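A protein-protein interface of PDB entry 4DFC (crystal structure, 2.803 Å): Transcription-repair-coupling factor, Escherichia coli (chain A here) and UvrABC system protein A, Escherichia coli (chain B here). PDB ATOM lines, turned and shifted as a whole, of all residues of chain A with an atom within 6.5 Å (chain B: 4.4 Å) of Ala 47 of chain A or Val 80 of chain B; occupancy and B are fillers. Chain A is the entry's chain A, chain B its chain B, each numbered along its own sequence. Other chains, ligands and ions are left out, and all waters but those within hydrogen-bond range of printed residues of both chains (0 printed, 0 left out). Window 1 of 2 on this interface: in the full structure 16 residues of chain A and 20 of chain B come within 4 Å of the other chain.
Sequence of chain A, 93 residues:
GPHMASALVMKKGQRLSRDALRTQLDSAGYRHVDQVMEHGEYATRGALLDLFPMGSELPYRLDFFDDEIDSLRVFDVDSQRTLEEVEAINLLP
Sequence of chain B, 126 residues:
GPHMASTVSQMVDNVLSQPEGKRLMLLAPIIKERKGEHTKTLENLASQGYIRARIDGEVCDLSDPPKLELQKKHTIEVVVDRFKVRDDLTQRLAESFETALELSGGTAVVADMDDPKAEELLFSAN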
ATOM      1  N   ARG A  18      12.828  16.807  10.385  1.00  0.00           N
ATOM      2  CA  ARG A  18      11.380  16.819  10.157  1.00  0.00           C
ATOM      3  C   ARG A  18      10.962  17.821   9.086  1.00  0.00           C
ATOM      4  O   ARG A  18      10.190  17.484   8.185  1.00  0.00           O
ATOM      5  CB  ARG A  18      10.605  17.072  11.456  1.00  0.00           C
ATOM      6  CG  ARG A  18      10.451  15.838  12.336  1.00  0.00           C
ATOM      7  CD  ARG A  18       9.566  14.804  11.683  1.00  0.00           C
ATOM      8  NE  ARG A  18       8.184  15.265  11.591  1.00  0.00           N
ATOM      9  CZ  ARG A  18       7.344  15.301  12.624  1.00  0.00           C
ATOM     10  NH1 ARG A  18       7.761  14.915  13.822  1.00  0.00           N
ATOM     11  NH2 ARG A  18       6.093  15.728  12.466  1.00  0.00           N
ATOM     12  N   ARG A  45       0.829  14.547  13.032  1.00  0.00           N
ATOM     13  CA  ARG A  45       0.313  14.590  14.386  1.00  0.00           C
ATOM     14  C   ARG A  45       1.498  14.510  15.338  1.00  0.00           C
ATOM     15  O   ARG A  45       1.991  13.410  15.595  1.00  0.00           O
ATOM     16  CB  ARG A  45      -0.512  13.321  14.583  1.00  0.00           C
ATOM     17  CG  ARG A  45      -1.974  13.516  14.763  1.00  0.00           C
ATOM     18  CD  ARG A  45      -2.687  12.257  14.373  1.00  0.00           C
ATOM     19  NE  ARG A  45      -2.907  12.185  12.936  1.00  0.00           N
ATOM     20  CZ  ARG A  45      -2.602  11.126  12.208  1.00  0.00           C
ATOM     21  NH1 ARG A  45      -2.061  10.078  12.810  1.00  0.00           N
ATOM     22  NH2 ARG A  45      -2.844  11.110  10.899  1.00  0.00           N
ATOM     23  N   GLY A  46       1.896  15.624  15.944  1.00  0.00           N
ATOM     24  CA  GLY A  46       3.023  15.581  16.867  1.00  0.00           C
ATOM     25  C   GLY A  46       4.269  14.869  16.322  1.00  0.00           C
ATOM     26  O   GLY A  46       4.836  15.210  15.270  1.00  0.00           O
ATOM     27  N   ALA A  47       4.691  13.861  17.083  1.00  0.00           N
ATOM     28  CA  ALA A  47       5.789  12.970  16.744  1.00  0.00           C
ATOM     29  C   ALA A  47       5.590  12.153  15.486  1.00  0.00           C
ATOM     30  O   ALA A  47       6.519  11.488  15.036  1.00  0.00           O
ATOM     31  CB  ALA A  47       6.042  12.020  17.904  1.00  0.00           C
ATOM     32  N   LEU A  48       4.377  12.158  14.945  1.00  0.00           N
ATOM     33  CA  LEU A  48       3.992  11.178  13.925  1.00  0.00           C
ATOM     34  C   LEU A  48       3.842  11.812  12.565  1.00  0.00           C
ATOM     35  O   LEU A  48       3.271  12.898  12.436  1.00  0.00           O
ATOM     36  CB  LEU A  48       2.667  10.492  14.282  1.00  0.00           C
ATOM     37  CG  LEU A  48       2.491   9.595  15.505  1.00  0.00           C
ATOM     38  CD1 LEU A  48       2.237  10.394  16.808  1.00  0.00           C
ATOM     39  CD2 LEU A  48       1.310   8.717  15.207  1.00  0.00           C
ATOM     40  N   LEU A  49       4.349  11.127  11.548  1.00  0.00           N
ATOM     41  CA  LEU A  49       4.142  11.560  10.172  1.00  0.00           C
ATOM     42  C   LEU A  49       3.585  10.412   9.344  1.00  0.00           C
ATOM     43  O   LEU A  49       4.295   9.440   9.088  1.00  0.00           O
ATOM     44  CB  LEU A  49       5.470  12.043   9.573  1.00  0.00           C
ATOM     45  CG  LEU A  49       5.410  12.714   8.201  1.00  0.00           C
ATOM     46  CD1 LEU A  49       6.228  14.001   8.177  1.00  0.00           C
ATOM     47  CD2 LEU A  49       5.869  11.762   7.127  1.00  0.00           C
ATOM     48  N   LEU A  62       5.321   6.916  10.631  1.00  0.00           N
ATOM     49  CA  LEU A  62       6.676   7.033  11.181  1.00  0.00           C
ATOM     50  C   LEU A  62       6.656   7.735  12.521  1.00  0.00           C
ATOM     51  O   LEU A  62       6.179   8.863  12.624  1.00  0.00           O
ATOM     52  CB  LEU A  62       7.567   7.840  10.229  1.00  0.00           C
ATOM     53  CG  LEU A  62       7.976   7.265   8.872  1.00  0.00           C
ATOM     54  CD1 LEU A  62       6.825   7.200   7.918  1.00  0.00           C
ATOM     55  CD2 LEU A  62       9.022   8.141   8.285  1.00  0.00           C
ATOM     56  N   ASP A  63       7.197   7.086  13.542  1.00  0.00           N
ATOM     57  CA  ASP A  63       7.193   7.667  14.881  1.00  0.00           C
ATOM     58  C   ASP A  63       8.522   8.370  15.174  1.00  0.00           C
ATOM     59  O   ASP A  63       9.575   7.722  15.277  1.00  0.00           O
ATOM     60  CB  ASP A  63       6.909   6.572  15.915  1.00  0.00           C
ATOM     61  CG  ASP A  63       6.613   7.118  17.304  1.00  0.00           C
ATOM     62  OD1 ASP A  63       6.332   8.323  17.445  1.00  0.00           O
ATOM     63  OD2 ASP A  63       6.655   6.318  18.264  1.00  0.00           O
ATOM     64  N   PHE A  64       8.480   9.697  15.304  1.00  0.00           N
ATOM     65  CA  PHE A  64       9.703  10.458  15.594  1.00  0.00           C
ATOM     66  C   PHE A  64       9.946  10.719  17.072  1.00  0.00           C
ATOM     67  O   PHE A  64       9.115  11.307  17.767  1.00  0.00           O
ATOM     68  CB  PHE A  64       9.744  11.781  14.825  1.00  0.00           C
ATOM     69  CG  PHE A  64      10.124  11.625  13.391  1.00  0.00           C
ATOM     70  CD1 PHE A  64       9.168  11.395  12.430  1.00  0.00           C
ATOM     71  CD2 PHE A  64      11.442  11.695  13.002  1.00  0.00           C
ATOM     72  CE1 PHE A  64       9.505  11.248  11.109  1.00  0.00           C
ATOM     73  CE2 PHE A  64      11.791  11.545  11.667  1.00  0.00           C
ATOM     74  CZ  PHE A  64      10.815  11.314  10.722  1.00  0.00           C
ATOM     75  N   PHE A  65      11.101  10.261  17.537  1.00  0.00           N
ATOM     76  CA  PHE A  65      11.624  10.638  18.847  1.00  0.00           C
ATOM     77  C   PHE A  65      12.722  11.666  18.587  1.00  0.00           C
ATOM     78  O   PHE A  65      13.776  11.332  18.042  1.00  0.00           O
ATOM     79  CB  PHE A  65      12.178   9.412  19.570  1.00  0.00           C
ATOM     80  CG  PHE A  65      12.533   9.660  21.004  1.00  0.00           C
ATOM     81  CD1 PHE A  65      12.348   8.665  21.954  1.00  0.00           C
ATOM     82  CD2 PHE A  65      13.072  10.873  21.403  1.00  0.00           C
ATOM     83  CE1 PHE A  65      12.685   8.890  23.282  1.00  0.00           C
ATOM     84  CE2 PHE A  65      13.414  11.102  22.723  1.00  0.00           C
ATOM     85  CZ  PHE A  65      13.221  10.115  23.663  1.00  0.00           C
ATOM     86  N   LEU B  26       5.283  15.106  25.727  1.00  0.00           N
ATOM     87  CA  LEU B  26       4.158  16.017  25.718  1.00  0.00           C
ATOM     88  C   LEU B  26       2.818  15.215  25.660  1.00  0.00           C
ATOM     89  O   LEU B  26       2.626  14.375  24.777  1.00  0.00           O
ATOM     90  CB  LEU B  26       4.323  16.973  24.543  1.00  0.00           C
ATOM     91  CG  LEU B  26       3.108  17.846  24.253  1.00  0.00           C
ATOM     92  CD1 LEU B  26       2.935  18.888  25.339  1.00  0.00           C
ATOM     93  CD2 LEU B  26       3.205  18.492  22.870  1.00  0.00           C
ATOM     94  N   ALA B  28      -1.643  14.947  25.901  1.00  0.00           N
ATOM     95  CA  ALA B  28      -3.005  15.501  25.924  1.00  0.00           C
ATOM     96  C   ALA B  28      -3.851  14.742  26.934  1.00  0.00           C
ATOM     97  O   ALA B  28      -4.100  13.540  26.760  1.00  0.00           O
ATOM     98  CB  ALA B  28      -3.646  15.416  24.559  1.00  0.00           C
ATOM     99  N   VAL B  78      -3.085  11.053  25.842  1.00  0.00           N
ATOM    100  CA  VAL B  78      -2.345  10.693  24.630  1.00  0.00           C
ATOM    101  C   VAL B  78      -0.894  11.175  24.714  1.00  0.00           C
ATOM    102  O   VAL B  78      -0.601  12.254  25.258  1.00  0.00           O
ATOM    103  CB  VAL B  78      -2.966  11.290  23.370  1.00  0.00           C
ATOM    104  CG1 VAL B  78      -2.289  10.689  22.143  1.00  0.00           C
ATOM    105  CG2 VAL B  78      -4.474  11.034  23.341  1.00  0.00           C
ATOM    106  N   VAL B  79       0.025  10.383  24.181  1.00  0.00           N
ATOM    107  CA  VAL B  79       1.376  10.884  24.068  1.00  0.00           C
ATOM    108  C   VAL B  79       1.523  11.477  22.671  1.00  0.00           C
ATOM    109  O   VAL B  79       1.754  10.755  21.701  1.00  0.00           O
ATOM    110  CB  VAL B  79       2.383   9.745  24.276  1.00  0.00           C
ATOM    111  CG1 VAL B  79       3.807  10.273  24.287  1.00  0.00           C
ATOM    112  CG2 VAL B  79       2.079   9.015  25.576  1.00  0.00           C
ATOM    113  N   VAL B  80       1.482  12.808  22.595  1.00  0.00           N
ATOM    114  CA  VAL B  80       1.559  13.529  21.325  1.00  0.00           C
ATOM    115  C   VAL B  80       2.979  13.581  20.775  1.00  0.00           C
ATOM    116  O   VAL B  80       3.171  13.528  19.567  1.00  0.00           O
ATOM    117  CB  VAL B  80       1.102  14.994  21.462  1.00  0.00           C
ATOM    118  CG1 VAL B  80       1.209  15.707  20.119  1.00  0.00           C
ATOM    119  CG2 VAL B  80      -0.313  15.094  22.011  1.00  0.00           C
ATOM    120  N   ASP B  81       3.968  13.716  21.662  1.00  0.00           N
ATOM    121  CA  ASP B  81       5.349  13.913  21.248  1.00  0.00           C
ATOM    122  C   ASP B  81       6.369  13.468  22.292  1.00  0.00           C
ATOM    123  O   ASP B  81       6.105  13.522  23.495  1.00  0.00           O
ATOM    124  CB  ASP B  81       5.583  15.392  20.931  1.00  0.00           C
ATOM    125  CG  ASP B  81       6.617  15.615  19.819  1.00  0.00           C
ATOM    126  OD1 ASP B  81       7.355  14.666  19.424  1.00  0.00           O
ATOM    127  OD2 ASP B  81       6.684  16.767  19.342  1.00  0.00           O
ATOM    128  N   ARG B  82       7.553  13.078  21.814  1.00  0.00           N
ATOM    129  CA  ARG B  82       8.664  12.701  22.671  1.00  0.00           C
ATOM    130  C   ARG B  82       9.953  13.396  22.185  1.00  0.00           C
ATOM    131  O   ARG B  82      10.392  13.165  21.060  1.00  0.00           O
ATOM    132  CB  ARG B  82       8.864  11.177  22.651  1.00  0.00           C
ATOM    133  CG  ARG B  82       7.608  10.335  22.656  1.00  0.00           C
ATOM    134  CD  ARG B  82       7.711   9.159  23.636  1.00  0.00           C
ATOM    135  NE  ARG B  82       8.249   7.875  23.142  1.00  0.00           N
ATOM    136  CZ  ARG B  82       8.511   7.545  21.876  1.00  0.00           C
ATOM    137  NH1 ARG B  82       8.307   8.399  20.876  1.00  0.00           N
ATOM    138  NH2 ARG B  82       8.991   6.335  21.614  1.00  0.00           N
ATOM    139  N   ARG B  92       8.510  22.836  15.365  1.00  0.00           N
ATOM    140  CA  ARG B  92       7.968  21.503  15.557  1.00  0.00           C
ATOM    141  C   ARG B  92       7.247  21.301  16.905  1.00  0.00           C
ATOM    142  O   ARG B  92       6.234  20.609  16.961  1.00  0.00           O
ATOM    143  CB  ARG B  92       9.132  20.513  15.481  1.00  0.00           C
ATOM    144  CG  ARG B  92       8.913  19.236  16.262  1.00  0.00           C
ATOM    145  CD  ARG B  92      10.226  18.558  16.640  1.00  0.00           C
ATOM    146  NE  ARG B  92      10.358  17.222  16.053  1.00  0.00           N
ATOM    147  CZ  ARG B  92       9.481  16.220  16.189  1.00  0.00           C
ATOM    148  NH1 ARG B  92       8.361  16.376  16.895  1.00  0.00           N
ATOM    149  NH2 ARG B  92       9.728  15.050  15.602  1.00  0.00           N
ATOM    150  N   SER B  96       3.253  20.522  17.836  1.00  0.00           N
ATOM    151  CA  SER B  96       2.929  19.462  18.762  1.00  0.00           C
ATOM    152  C   SER B  96       2.088  19.933  19.959  1.00  0.00           C
ATOM    153  O   SER B  96       1.205  19.221  20.408  1.00  0.00           O
ATOM    154  CB  SER B  96       4.208  18.763  19.195  1.00  0.00           C
ATOM    155  OG  SER B  96       4.826  18.214  18.046  1.00  0.00           O
ATOM    156  N   THR B  99      -1.507  20.715  18.575  1.00  0.00           N
ATOM    157  CA  THR B  99      -2.130  19.415  18.466  1.00  0.00           C
ATOM    158  C   THR B  99      -2.603  18.844  19.821  1.00  0.00           C
ATOM    159  O   THR B  99      -3.703  18.310  19.932  1.00  0.00           O
ATOM    160  CB  THR B  99      -1.177  18.438  17.762  1.00  0.00           C
ATOM    161  OG1 THR B  99      -1.122  18.767  16.373  1.00  0.00           O
ATOM    162  CG2 THR B  99      -1.670  17.024  17.890  1.00  0.00           C
ATOM    163  N   ALA B 100      -1.785  18.953  20.852  1.00  0.00           N
ATOM    164  CA  ALA B 100      -2.163  18.402  22.138  1.00  0.00           C
ATOM    165  C   ALA B 100      -3.329  19.204  22.679  1.00  0.00           C
ATOM    166  O   ALA B 100      -4.227  18.665  23.329  1.00  0.00           O
ATOM    167  CB  ALA B 100      -0.986  18.457  23.106  1.00  0.00           C
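The guanidinium group of Arg 18 of chain A lies close to the guanidinium group of Arg 92 of chain B. The backbone carbonyl oxygen of Val 80 of chain B lies within hydrogen-bond range of the backbone NH of Ala 47 of chain A, 2.9 Å away. The side-chain carboxylate (OD2) of Asp 63 of chain A is in salt-bridge range of the guanidinium group (NH1) of Arg 82 of chain B, 3.7 Å away.
The guanidinium group (NH2) of Arg 18 of chain A is in hydrogen-bond range of the backbone carbonyl oxygen (O) of Gly 46 of chain A, at 3.1 Å. The backbone NH (N) of Phe 64 of chain A is in hydrogen-bond range of the backbone carbonyl oxygen (O) of Ala 47 of chain A (2.7 Å). O of Leu 26 of chain B is in hydrogen-bond range of N of Val 80 of chain B (2.9 Å). The backbone NH (N) of Leu 26 of chain B is in hydrogen-bond range of the backbone carbonyl oxygen (O) of Asp 81 of chain B (2.9 Å). NH1 of Arg 92 of chain B lies within salt-bridge range of OD2 of Asp 81 of chain B, 3.0 Å away. The side-chain carboxylate (OD2) of Asp 81 of chain B lies within hydrogen-bond range of the side-chain hydroxyl (OG) of Ser 96 of chain B (2.7 Å).
O of Val 80 of chain B touches CA of Gly 46 of chain A (3.4 Å). Gly 46 of chain A touches Ser 96 of chain B. Ala 47 of chain A touches Asp 81 of chain B. Arg 82 of chain B touches Phe 64 of chain A (O to O, 3.99 Å). Phe 64 of chain A touches Arg 92 of chain B (CB to NH2, 3.4 Å). Phe 65 of chain A touches Arg 82 of chain B (CD2 to O, 3.5 Å).
Arg 45 of chain A touches none of the printed residues of chain B. Ala 47 of chain A touches just these residues of chain B: Val 80 and Asp 81. Of the printed residues of chain B, Phe 64 of chain A touches Arg 82 (3.99 Å) and Arg 92 (3.4 Å). Val 80 of chain B touches just these residues of chain A: Gly 46 (3.4 Å) and Ala 47 (2.9 Å). Of the printed residues of chain A, Ser 96 of chain B touches Gly 46 (3.4 Å). The nearest residue of chain A that does not touch Val 80 of chain B is Arg 45 of chain A (4.1 Å).
Among the printed residues, Asp or Glu carboxylates within 4 Å of a Lys or Arg side-chain nitrogen of the other chain: Asp 63 of chain A with Arg 82 of chain B (3.7 Å).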
